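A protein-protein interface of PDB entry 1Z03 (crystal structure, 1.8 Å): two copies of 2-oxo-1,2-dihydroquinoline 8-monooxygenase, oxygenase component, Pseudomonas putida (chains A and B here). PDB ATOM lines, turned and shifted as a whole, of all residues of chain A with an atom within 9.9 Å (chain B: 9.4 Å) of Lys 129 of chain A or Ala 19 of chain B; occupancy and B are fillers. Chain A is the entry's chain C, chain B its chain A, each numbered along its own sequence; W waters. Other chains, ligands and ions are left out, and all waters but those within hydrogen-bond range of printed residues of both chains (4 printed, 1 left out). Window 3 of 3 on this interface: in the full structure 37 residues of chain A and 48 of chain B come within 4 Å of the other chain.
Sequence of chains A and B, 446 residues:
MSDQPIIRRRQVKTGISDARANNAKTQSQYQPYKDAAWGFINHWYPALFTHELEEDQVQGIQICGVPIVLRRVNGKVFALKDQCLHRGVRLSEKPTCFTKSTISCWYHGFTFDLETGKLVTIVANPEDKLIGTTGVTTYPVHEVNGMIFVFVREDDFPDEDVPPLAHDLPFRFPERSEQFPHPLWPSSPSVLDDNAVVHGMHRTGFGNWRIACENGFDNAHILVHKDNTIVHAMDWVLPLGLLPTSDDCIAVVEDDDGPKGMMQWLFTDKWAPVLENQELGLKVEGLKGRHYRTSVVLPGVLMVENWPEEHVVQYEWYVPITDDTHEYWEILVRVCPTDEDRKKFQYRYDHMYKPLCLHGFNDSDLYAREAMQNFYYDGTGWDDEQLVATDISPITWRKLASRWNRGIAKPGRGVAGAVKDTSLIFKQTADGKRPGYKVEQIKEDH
The side-chain hydroxyl (OG) of Ser 17 of chain B sits at hydrogen-bond distance from the side-chain hydroxyl (OG1) of Thr 133 of chain A, at 2.6 Å. The backbone carbonyl oxygen (O) of Ala 19 of chain B lies within hydrogen-bond range of the side-chain amino group (NZ) of Lys 129 of chain A. The backbone NH (N) of Gln 386 of chain B sits close to the backbone carbonyl oxygen (O) of Leu 85 of chain A. The backbone NH of Ala 389 of chain B is in hydrogen-bond range of the side-chain carboxylate of Asp 128 of chain A (2.9 Å).
The backbone NH of Ser 17 of chain B sits at hydrogen-bond distance from the side-chain amide oxygen of Gln 386 of chain B (3.0 Å). The guanidinium group of Arg 20 of chain B sits at hydrogen-bond distance from the backbone carbonyl oxygen of Glu 385 of chain B (2.7 Å). N of Val 388 of chain B is in hydrogen-bond range of OD1 of Asp 391 of chain B, at 2.8 Å. O of Thr 134 of chain A sits at hydrogen-bond distance from N of Leu 119 of chain A. The side-chain amide nitrogen (ND2) of Asn 125 of chain A lies within hydrogen-bond range of the side-chain carboxylate (OD1) of Asp 128 of chain A, 3.0 Å away. N of Leu 130 of chain A sits at hydrogen-bond distance from OD2 of Asp 128 of chain A (2.9 Å).
Val 388 of chain B touches Phe 110 of chain A (CG1 to CZ, 3.6 Å). Asn 125 of chain A touches Val 388 of chain B. CB of Ala 389 of chain B touches ND2 of Asn 125 of chain A, 3.95 Å away. Asp 128 of chain A touches Val 388 of chain B. OG of Ser 17 of chain B touches CD1 of Leu 130 of chain A, at 3.5 Å. Ala 19 of chain B touches Leu 130 of chain A (CB to CA, 3.8 Å). Leu 130 of chain A touches Gln 386 of chain B (CD2 to O, 3.9 Å). CG1 of Val 388 of chain B touches CD2 of Leu 130 of chain A, 3.5 Å away. Ser 17 of chain B touches Thr 134 of chain A (CB to CB, 3.9 Å). Gln 386 of chain B touches Thr 134 of chain A (OE1 to CG2, 3.8 Å).
Lys 129 of chain A touches just one residue of chain B: Ala 19 (3.4 Å). Asp 128 of chain A touches just these residues of chain B: Val 388 (3.2 Å) and Ala 389 (2.9 Å). Of chain A, only Leu 130, Thr 133 and Thr 134 come within 4 Å of Ser 17 of chain B. Of the printed residues of chain A, Val 388 of chain B touches Phe 110 (3.6 Å), Asn 125 (3.99 Å), Asp 128 (3.2 Å) and Leu 130 (3.5 Å). Of the printed residues of chain B, Leu 85 of chain A touches Gln 386 (3.4 Å). Printed residues of chain B within 4 Å of Leu 130 of chain A: Ser 17 (3.5 Å), Ala 19 (3.8 Å), Arg 20 (3.7 Å), Gln 386 (3.9 Å) and Val 388 (3.5 Å). Val 120 of chain A touches none of the printed residues of chain B.
Of the 16 printed residues of chain B, 6 touch a printed residue of chain A. Hydrophobic or aromatic side chains of chain B that line the printed part of chain A: Ala 19, Val 388 and Ala 389. Of the 16 printed residues of chain A, 8 touch a printed residue of chain B. Hydrophobic or aromatic side chains of chain A within 4 Å of the printed part of chain B: Leu 85, Phe 110 and Leu 130. Among the printed residues, no Asp or Glu carboxylate lies within 4 Å of a Lys or Arg side-chain nitrogen of the other chain.
No position is printed for both chains.
Water W2 bridges O of Leu 85 of chain A and NE2 of Gln 386 of chain B. Water W1 lies within hydrogen-bond range of the side-chain carboxylate of Asp 128 of chain A (2.8 Å) and the backbone carbonyl oxygen of Ala 19 of chain B (2.9 Å). Water W3 lies within hydrogen-bond range of OG1 of Thr 390 of chain B (2.8 Å) and ND2 of Asn 125 of chain A (3.0 Å). Water W4 bridges the backbone NH (N) of Ala 389 of chain B and the side-chain amino group (NZ) of Lys 129 of chain A.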
ATOM      1  N   LEU A  85     -16.974  -1.225 -10.901  1.00  0.00           N
ATOM      2  CA  LEU A  85     -16.910  -2.389 -10.031  1.00  0.00           C
ATOM      3  C   LEU A  85     -17.971  -3.453 -10.332  1.00  0.00           C
ATOM      4  O   LEU A  85     -17.923  -4.556  -9.782  1.00  0.00           O
ATOM      5  CB  LEU A  85     -16.965  -1.937  -8.562  1.00  0.00           C
ATOM      6  CG  LEU A  85     -18.178  -1.176  -8.004  1.00  0.00           C
ATOM      7  CD1 LEU A  85     -19.325  -2.155  -7.742  1.00  0.00           C
ATOM      8  CD2 LEU A  85     -17.780  -0.469  -6.707  1.00  0.00           C
ATOM      9  N   PHE A 110     -24.236   1.985 -12.914  1.00  0.00           N
ATOM     10  CA  PHE A 110     -23.656   2.125 -11.581  1.00  0.00           C
ATOM     11  C   PHE A 110     -23.141   3.559 -11.499  1.00  0.00           C
ATOM     12  O   PHE A 110     -22.481   4.028 -12.424  1.00  0.00           O
ATOM     13  CB  PHE A 110     -22.510   1.133 -11.380  1.00  0.00           C
ATOM     14  CG  PHE A 110     -22.958  -0.221 -10.892  1.00  0.00           C
ATOM     15  CD1 PHE A 110     -24.070  -0.849 -11.454  1.00  0.00           C
ATOM     16  CD2 PHE A 110     -22.258  -0.877  -9.888  1.00  0.00           C
ATOM     17  CE1 PHE A 110     -24.475  -2.107 -11.020  1.00  0.00           C
ATOM     18  CE2 PHE A 110     -22.655  -2.139  -9.448  1.00  0.00           C
ATOM     19  CZ  PHE A 110     -23.763  -2.755 -10.015  1.00  0.00           C
ATOM     20  N   LEU A 119     -20.274   3.914  -4.254  1.00  0.00           N
ATOM     21  CA  LEU A 119     -21.376   3.603  -5.161  1.00  0.00           C
ATOM     22  C   LEU A 119     -22.601   4.229  -4.487  1.00  0.00           C
ATOM     23  O   LEU A 119     -23.110   3.703  -3.491  1.00  0.00           O
ATOM     24  CB  LEU A 119     -21.557   2.082  -5.283  1.00  0.00           C
ATOM     25  CG  LEU A 119     -22.759   1.578  -6.088  1.00  0.00           C
ATOM     26  CD1 LEU A 119     -22.730   2.175  -7.488  1.00  0.00           C
ATOM     27  CD2 LEU A 119     -22.742   0.055  -6.150  1.00  0.00           C
ATOM     28  N   VAL A 120     -23.055   5.360  -5.024  1.00  0.00           N
ATOM     29  CA  VAL A 120     -24.195   6.074  -4.459  1.00  0.00           C
ATOM     30  C   VAL A 120     -25.552   5.627  -4.980  1.00  0.00           C
ATOM     31  O   VAL A 120     -26.562   5.813  -4.304  1.00  0.00           O
ATOM     32  CB  VAL A 120     -24.050   7.595  -4.673  1.00  0.00           C
ATOM     33  CG1 VAL A 120     -22.832   8.102  -3.920  1.00  0.00           C
ATOM     34  CG2 VAL A 120     -23.913   7.909  -6.150  1.00  0.00           C
ATOM     35  N   THR A 121     -25.588   5.048  -6.179  1.00  0.00           N
ATOM     36  CA  THR A 121     -26.849   4.569  -6.744  1.00  0.00           C
ATOM     37  C   THR A 121     -26.622   3.827  -8.060  1.00  0.00           C
ATOM     38  O   THR A 121     -25.489   3.697  -8.524  1.00  0.00           O
ATOM     39  CB  THR A 121     -27.852   5.735  -6.990  1.00  0.00           C
ATOM     40  OG1 THR A 121     -29.129   5.209  -7.379  1.00  0.00           O
ATOM     41  CG2 THR A 121     -27.349   6.654  -8.088  1.00  0.00           C
ATOM     42  N   ILE A 122     -27.713   3.325  -8.631  1.00  0.00           N
ATOM     43  CA  ILE A 122     -27.702   2.608  -9.901  1.00  0.00           C
ATOM     44  C   ILE A 122     -28.921   3.158 -10.642  1.00  0.00           C
ATOM     45  O   ILE A 122     -30.052   2.993 -10.187  1.00  0.00           O
ATOM     46  CB  ILE A 122     -27.858   1.078  -9.695  1.00  0.00           C
ATOM     47  CG1 ILE A 122     -26.679   0.535  -8.883  1.00  0.00           C
ATOM     48  CG2 ILE A 122     -27.934   0.369 -11.050  1.00  0.00           C
ATOM     49  CD1 ILE A 122     -26.805  -0.936  -8.515  1.00  0.00           C
ATOM     50  N   ASN A 125     -31.902   0.837 -10.876  1.00  0.00           N
ATOM     51  CA  ASN A 125     -31.969  -0.116  -9.765  1.00  0.00           C
ATOM     52  C   ASN A 125     -31.493   0.600  -8.503  1.00  0.00           C
ATOM     53  O   ASN A 125     -30.573   0.148  -7.819  1.00  0.00           O
ATOM     54  CB  ASN A 125     -31.084  -1.330 -10.065  1.00  0.00           C
ATOM     55  CG  ASN A 125     -31.208  -2.417  -9.021  1.00  0.00           C
ATOM     56  OD1 ASN A 125     -32.100  -2.383  -8.170  1.00  0.00           O
ATOM     57  ND2 ASN A 125     -30.319  -3.403  -9.088  1.00  0.00           N
ATOM     58  N   PRO A 126     -32.145   1.728  -8.170  1.00  0.00           N
ATOM     59  CA  PRO A 126     -31.841   2.568  -7.007  1.00  0.00           C
ATOM     60  C   PRO A 126     -31.932   1.936  -5.617  1.00  0.00           C
ATOM     61  O   PRO A 126     -31.377   2.481  -4.663  1.00  0.00           O
ATOM     62  CB  PRO A 126     -32.821   3.730  -7.166  1.00  0.00           C
ATOM     63  CG  PRO A 126     -34.021   3.051  -7.759  1.00  0.00           C
ATOM     64  CD  PRO A 126     -33.390   2.184  -8.821  1.00  0.00           C
ATOM     65  N   GLU A 127     -32.612   0.802  -5.494  1.00  0.00           N
ATOM     66  CA  GLU A 127     -32.759   0.178  -4.185  1.00  0.00           C
ATOM     67  C   GLU A 127     -31.924  -1.070  -3.963  1.00  0.00           C
ATOM     68  O   GLU A 127     -32.096  -1.755  -2.957  1.00  0.00           O
ATOM     69  CB  GLU A 127     -34.236  -0.136  -3.940  1.00  0.00           C
ATOM     70  CG  GLU A 127     -35.114   1.099  -4.104  1.00  0.00           C
ATOM     71  CD  GLU A 127     -36.498   0.942  -3.516  1.00  0.00           C
ATOM     72  OE1 GLU A 127     -37.183   1.966  -3.343  1.00  0.00           O
ATOM     73  OE2 GLU A 127     -36.911  -0.194  -3.235  1.00  0.00           O
ATOM     74  N   ASP A 128     -31.007  -1.363  -4.881  1.00  0.00           N
ATOM     75  CA  ASP A 128     -30.187  -2.561  -4.723  1.00  0.00           C
ATOM     76  C   ASP A 128     -29.390  -2.501  -3.428  1.00  0.00           C
ATOM     77  O   ASP A 128     -28.855  -1.451  -3.063  1.00  0.00           O
ATOM     78  CB  ASP A 128     -29.216  -2.749  -5.890  1.00  0.00           C
ATOM     79  CG  ASP A 128     -28.708  -4.181  -5.985  1.00  0.00           C
ATOM     80  OD1 ASP A 128     -29.366  -4.993  -6.670  1.00  0.00           O
ATOM     81  OD2 ASP A 128     -27.672  -4.499  -5.355  1.00  0.00           O
ATOM     82  N   LYS A 129     -29.305  -3.642  -2.748  1.00  0.00           N
ATOM     83  CA  LYS A 129     -28.583  -3.738  -1.492  1.00  0.00           C
ATOM     84  C   LYS A 129     -27.077  -3.512  -1.626  1.00  0.00           C
ATOM     85  O   LYS A 129     -26.400  -3.275  -0.629  1.00  0.00           O
ATOM     86  CB  LYS A 129     -28.844  -5.098  -0.833  1.00  0.00           C
ATOM     87  CG  LYS A 129     -28.409  -6.321  -1.646  1.00  0.00           C
ATOM     88  CD  LYS A 129     -28.210  -7.512  -0.714  1.00  0.00           C
ATOM     89  CE  LYS A 129     -29.066  -8.707  -1.090  1.00  0.00           C
ATOM     90  NZ  LYS A 129     -28.453  -9.491  -2.186  1.00  0.00           N
ATOM     91  N   LEU A 130     -26.546  -3.581  -2.844  1.00  0.00           N
ATOM     92  CA  LEU A 130     -25.112  -3.374  -3.035  1.00  0.00           C
ATOM     93  C   LEU A 130     -24.744  -1.909  -2.907  1.00  0.00           C
ATOM     94  O   LEU A 130     -23.615  -1.569  -2.556  1.00  0.00           O
ATOM     95  CB  LEU A 130     -24.667  -3.862  -4.414  1.00  0.00           C
ATOM     96  CG  LEU A 130     -23.158  -3.771  -4.697  1.00  0.00           C
ATOM     97  CD1 LEU A 130     -22.416  -4.865  -3.925  1.00  0.00           C
ATOM     98  CD2 LEU A 130     -22.904  -3.927  -6.193  1.00  0.00           C
ATOM     99  N   ILE A 131     -25.708  -1.041  -3.197  1.00  0.00           N
ATOM    100  CA  ILE A 131     -25.486   0.399  -3.146  1.00  0.00           C
ATOM    101  C   ILE A 131     -25.018   0.862  -1.775  1.00  0.00           C
ATOM    102  O   ILE A 131     -25.589   0.474  -0.755  1.00  0.00           O
ATOM    103  CB  ILE A 131     -26.772   1.164  -3.536  1.00  0.00           C
ATOM    104  CG1 ILE A 131     -27.128   0.860  -4.992  1.00  0.00           C
ATOM    105  CG2 ILE A 131     -26.573   2.660  -3.332  1.00  0.00           C
ATOM    106  CD1 ILE A 131     -28.462   1.403  -5.439  1.00  0.00           C
ATOM    107  N   GLY A 132     -23.969   1.684  -1.772  1.00  0.00           N
ATOM    108  CA  GLY A 132     -23.423   2.221  -0.541  1.00  0.00           C
ATOM    109  C   GLY A 132     -22.501   1.293   0.224  1.00  0.00           C
ATOM    110  O   GLY A 132     -21.791   1.733   1.130  1.00  0.00           O
ATOM    111  N   THR A 133     -22.491   0.014  -0.141  1.00  0.00           N
ATOM    112  CA  THR A 133     -21.660  -0.961   0.556  1.00  0.00           C
ATOM    113  C   THR A 133     -20.252  -1.078  -0.010  1.00  0.00           C
ATOM    114  O   THR A 133     -19.420  -1.809   0.533  1.00  0.00           O
ATOM    115  CB  THR A 133     -22.303  -2.363   0.540  1.00  0.00           C
ATOM    116  OG1 THR A 133     -22.267  -2.894  -0.789  1.00  0.00           O
ATOM    117  CG2 THR A 133     -23.744  -2.296   1.004  1.00  0.00           C
ATOM    118  N   THR A 134     -19.982  -0.365  -1.101  1.00  0.00           N
ATOM    119  CA  THR A 134     -18.667  -0.397  -1.733  1.00  0.00           C
ATOM    120  C   THR A 134     -18.486   0.805  -2.659  1.00  0.00           C
ATOM    121  O   THR A 134     -19.357   1.672  -2.736  1.00  0.00           O
ATOM    122  CB  THR A 134     -18.474  -1.721  -2.533  1.00  0.00           C
ATOM    123  OG1 THR A 134     -17.185  -1.722  -3.160  1.00  0.00           O
ATOM    124  CG2 THR A 134     -19.554  -1.883  -3.591  1.00  0.00           C
ATOM    125  N   ILE B  16     -14.521  -5.886  -2.582  1.00  0.00           N
ATOM    126  CA  ILE B  16     -15.688  -6.731  -2.972  1.00  0.00           C
ATOM    127  C   ILE B  16     -16.699  -6.847  -1.824  1.00  0.00           C
ATOM    128  O   ILE B  16     -16.391  -7.375  -0.756  1.00  0.00           O
ATOM    129  CB  ILE B  16     -15.215  -8.136  -3.416  1.00  0.00           C
ATOM    130  CG1 ILE B  16     -14.359  -8.000  -4.676  1.00  0.00           C
ATOM    131  CG2 ILE B  16     -16.400  -9.045  -3.671  1.00  0.00           C
ATOM    132  CD1 ILE B  16     -13.774  -9.292  -5.156  1.00  0.00           C
ATOM    133  N   SER B  17     -17.905  -6.340  -2.066  1.00  0.00           N
ATOM    134  CA  SER B  17     -18.990  -6.336  -1.085  1.00  0.00           C
ATOM    135  C   SER B  17     -19.765  -7.652  -0.963  1.00  0.00           C
ATOM    136  O   SER B  17     -19.950  -8.376  -1.939  1.00  0.00           O
ATOM    137  CB  SER B  17     -19.962  -5.195  -1.420  1.00  0.00           C
ATOM    138  OG  SER B  17     -21.161  -5.277  -0.669  1.00  0.00           O
ATOM    139  N   ASP B  18     -20.228  -7.937   0.253  1.00  0.00           N
ATOM    140  CA  ASP B  18     -20.994  -9.147   0.546  1.00  0.00           C
ATOM    141  C   ASP B  18     -22.432  -9.037   0.061  1.00  0.00           C
ATOM    142  O   ASP B  18     -23.180 -10.017   0.087  1.00  0.00           O
ATOM    143  CB  ASP B  18     -21.012  -9.409   2.051  1.00  0.00           C
ATOM    144  CG  ASP B  18     -19.627  -9.599   2.626  1.00  0.00           C
ATOM    145  OD1 ASP B  18     -19.509  -9.669   3.868  1.00  0.00           O
ATOM    146  OD2 ASP B  18     -18.657  -9.683   1.838  1.00  0.00           O
ATOM    147  N   ALA B  19     -22.821  -7.844  -0.372  1.00  0.00           N
ATOM    148  CA  ALA B  19     -24.176  -7.624  -0.850  1.00  0.00           C
ATOM    149  C   ALA B  19     -24.345  -7.966  -2.332  1.00  0.00           C
ATOM    150  O   ALA B  19     -25.444  -7.851  -2.869  1.00  0.00           O
ATOM    151  CB  ALA B  19     -24.584  -6.179  -0.591  1.00  0.00           C
ATOM    152  N   ARG B  20     -23.269  -8.391  -2.993  1.00  0.00           N
ATOM    153  CA  ARG B  20     -23.357  -8.737  -4.412  1.00  0.00           C
ATOM    154  C   ARG B  20     -24.141 -10.031  -4.578  1.00  0.00           C
ATOM    155  O   ARG B  20     -24.101 -10.893  -3.708  1.00  0.00           O
ATOM    156  CB  ARG B  20     -21.956  -8.869  -5.037  1.00  0.00           C
ATOM    157  CG  ARG B  20     -21.105 -10.017  -4.525  1.00  0.00           C
ATOM    158  CD  ARG B  20     -19.766 -10.070  -5.267  1.00  0.00           C
ATOM    159  NE  ARG B  20     -18.892 -11.127  -4.756  1.00  0.00           N
ATOM    160  CZ  ARG B  20     -17.789 -11.555  -5.366  1.00  0.00           C
ATOM    161  NH1 ARG B  20     -17.409 -11.020  -6.515  1.00  0.00           N
ATOM    162  NH2 ARG B  20     -17.070 -12.533  -4.831  1.00  0.00           N
ATOM    163  N   ALA B  21     -24.848 -10.165  -5.696  1.00  0.00           N
ATOM    164  CA  ALA B  21     -25.660 -11.348  -5.971  1.00  0.00           C
ATOM    165  C   ALA B  21     -24.865 -12.614  -6.263  1.00  0.00           C
ATOM    166  O   ALA B  21     -25.358 -13.721  -6.026  1.00  0.00           O
ATOM    167  CB  ALA B  21     -26.607 -11.066  -7.137  1.00  0.00           C
ATOM    168  N   ASN B  22     -23.653 -12.469  -6.794  1.00  0.00           N
ATOM    169  CA  ASN B  22     -22.845 -13.641  -7.108  1.00  0.00           C
ATOM    170  C   ASN B  22     -21.958 -14.062  -5.945  1.00  0.00           C
ATOM    171  O   ASN B  22     -20.739 -13.895  -5.979  1.00  0.00           O
ATOM    172  CB  ASN B  22     -21.981 -13.408  -8.364  1.00  0.00           C
ATOM    173  CG  ASN B  22     -21.055 -12.206  -8.234  1.00  0.00           C
ATOM    174  OD1 ASN B  22     -19.907 -12.237  -8.697  1.00  0.00           O
ATOM    175  ND2 ASN B  22     -21.554 -11.137  -7.625  1.00  0.00           N
ATOM    176  N   ASN B  23     -22.586 -14.616  -4.915  1.00  0.00           N
ATOM    177  CA  ASN B  23     -21.868 -15.079  -3.738  1.00  0.00           C
ATOM    178  C   ASN B  23     -21.226 -16.420  -4.048  1.00  0.00           C
ATOM    179  O   ASN B  23     -21.501 -17.010  -5.097  1.00  0.00           O
ATOM    180  CB  ASN B  23     -22.827 -15.187  -2.545  1.00  0.00           C
ATOM    181  CG  ASN B  23     -24.093 -15.958  -2.874  1.00  0.00           C
ATOM    182  OD1 ASN B  23     -25.183 -15.598  -2.426  1.00  0.00           O
ATOM    183  ND2 ASN B  23     -23.956 -17.028  -3.648  1.00  0.00           N
ATOM    184  N   THR B  26     -23.438 -19.247  -5.166  1.00  0.00           N
ATOM    185  CA  THR B  26     -23.955 -19.002  -6.506  1.00  0.00           C
ATOM    186  C   THR B  26     -22.888 -19.283  -7.569  1.00  0.00           C
ATOM    187  O   THR B  26     -23.146 -19.977  -8.551  1.00  0.00           O
ATOM    188  CB  THR B  26     -24.460 -17.544  -6.644  1.00  0.00           C
ATOM    189  OG1 THR B  26     -25.560 -17.339  -5.747  1.00  0.00           O
ATOM    190  CG2 THR B  26     -24.932 -17.260  -8.070  1.00  0.00           C
ATOM    191  N   GLU B 385     -16.317  -9.827 -10.341  1.00  0.00           N
ATOM    192  CA  GLU B 385     -17.469  -9.040 -10.761  1.00  0.00           C
ATOM    193  C   GLU B 385     -18.406  -8.906  -9.546  1.00  0.00           C
ATOM    194  O   GLU B 385     -18.463  -9.806  -8.693  1.00  0.00           O
ATOM    195  CB  GLU B 385     -18.201  -9.744 -11.916  1.00  0.00           C
ATOM    196  CG  GLU B 385     -18.817 -11.089 -11.527  1.00  0.00           C
ATOM    197  CD  GLU B 385     -19.378 -11.866 -12.706  1.00  0.00           C
ATOM    198  OE1 GLU B 385     -19.551 -11.294 -13.800  1.00  0.00           O
ATOM    199  OE2 GLU B 385     -19.656 -13.070 -12.530  1.00  0.00           O
ATOM    200  N   GLN B 386     -19.112  -7.781  -9.447  1.00  0.00           N
ATOM    201  CA  GLN B 386     -20.048  -7.587  -8.341  1.00  0.00           C
ATOM    202  C   GLN B 386     -21.445  -7.400  -8.907  1.00  0.00           C
ATOM    203  O   GLN B 386     -21.903  -6.281  -9.139  1.00  0.00           O
ATOM    204  CB  GLN B 386     -19.623  -6.396  -7.480  1.00  0.00           C
ATOM    205  CG  GLN B 386     -18.254  -6.624  -6.837  1.00  0.00           C
ATOM    206  CD  GLN B 386     -17.878  -5.570  -5.814  1.00  0.00           C
ATOM    207  OE1 GLN B 386     -18.579  -5.379  -4.823  1.00  0.00           O
ATOM    208  NE2 GLN B 386     -16.762  -4.883  -6.046  1.00  0.00           N
ATOM    209  N   LEU B 387     -22.112  -8.532  -9.125  1.00  0.00           N
ATOM    210  CA  LEU B 387     -23.450  -8.578  -9.700  1.00  0.00           C
ATOM    211  C   LEU B 387     -24.537  -8.122  -8.744  1.00  0.00           C
ATOM    212  O   LEU B 387     -24.377  -8.189  -7.525  1.00  0.00           O
ATOM    213  CB  LEU B 387     -23.748  -9.998 -10.191  1.00  0.00           C
ATOM    214  CG  LEU B 387     -22.670 -10.558 -11.129  1.00  0.00           C
ATOM    215  CD1 LEU B 387     -23.121 -11.904 -11.703  1.00  0.00           C
ATOM    216  CD2 LEU B 387     -22.394  -9.550 -12.259  1.00  0.00           C
ATOM    217  N   VAL B 388     -25.643  -7.660  -9.317  1.00  0.00           N
ATOM    218  CA  VAL B 388     -26.772  -7.172  -8.541  1.00  0.00           C
ATOM    219  C   VAL B 388     -28.083  -7.841  -8.943  1.00  0.00           C
ATOM    220  O   VAL B 388     -28.084  -8.805  -9.709  1.00  0.00           O
ATOM    221  CB  VAL B 388     -26.901  -5.639  -8.666  1.00  0.00           C
ATOM    222  CG1 VAL B 388     -25.731  -4.967  -7.948  1.00  0.00           C
ATOM    223  CG2 VAL B 388     -26.935  -5.232 -10.141  1.00  0.00           C
ATOM    224  N   ALA B 389     -29.198  -7.318  -8.437  1.00  0.00           N
ATOM    225  CA  ALA B 389     -30.516  -7.896  -8.698  1.00  0.00           C
ATOM    226  C   ALA B 389     -30.849  -8.187 -10.158  1.00  0.00           C
ATOM    227  O   ALA B 389     -31.380  -9.249 -10.477  1.00  0.00           O
ATOM    228  CB  ALA B 389     -31.608  -7.005  -8.088  1.00  0.00           C
ATOM    229  N   THR B 390     -30.558  -7.241 -11.045  1.00  0.00           N
ATOM    230  CA  THR B 390     -30.856  -7.437 -12.460  1.00  0.00           C
ATOM    231  C   THR B 390     -30.009  -8.539 -13.091  1.00  0.00           C
ATOM    232  O   THR B 390     -30.314  -9.024 -14.178  1.00  0.00           O
ATOM    233  CB  THR B 390     -30.644  -6.138 -13.246  1.00  0.00           C
ATOM    234  OG1 THR B 390     -29.380  -5.562 -12.884  1.00  0.00           O
ATOM    235  CG2 THR B 390     -31.761  -5.152 -12.942  1.00  0.00           C
ATOM    236  N   ASP B 391     -28.949  -8.948 -12.407  1.00  0.00           N
ATOM    237  CA  ASP B 391     -28.084  -9.983 -12.939  1.00  0.00           C
ATOM    238  C   ASP B 391     -28.640 -11.386 -12.769  1.00  0.00           C
ATOM    239  O   ASP B 391     -27.967 -12.373 -13.063  1.00  0.00           O
ATOM    240  CB  ASP B 391     -26.702  -9.844 -12.326  1.00  0.00           C
ATOM    241  CG  ASP B 391     -25.979  -8.632 -12.857  1.00  0.00           C
ATOM    242  OD1 ASP B 391     -25.359  -7.894 -12.066  1.00  0.00           O
ATOM    243  OD2 ASP B 391     -26.041  -8.421 -14.089  1.00  0.00           O
HETATM  244  O   HOH W   1     -27.204  -7.207  -5.054  1.00  0.00           O
HETATM  245  O   HOH W   2     -15.631  -5.584  -8.842  1.00  0.00           O
HETATM  246  O   HOH W   3     -29.096  -3.022 -11.762  1.00  0.00           O
HETATM  247  O   HOH W   4     -29.316  -8.392  -5.367  1.00  0.00           O
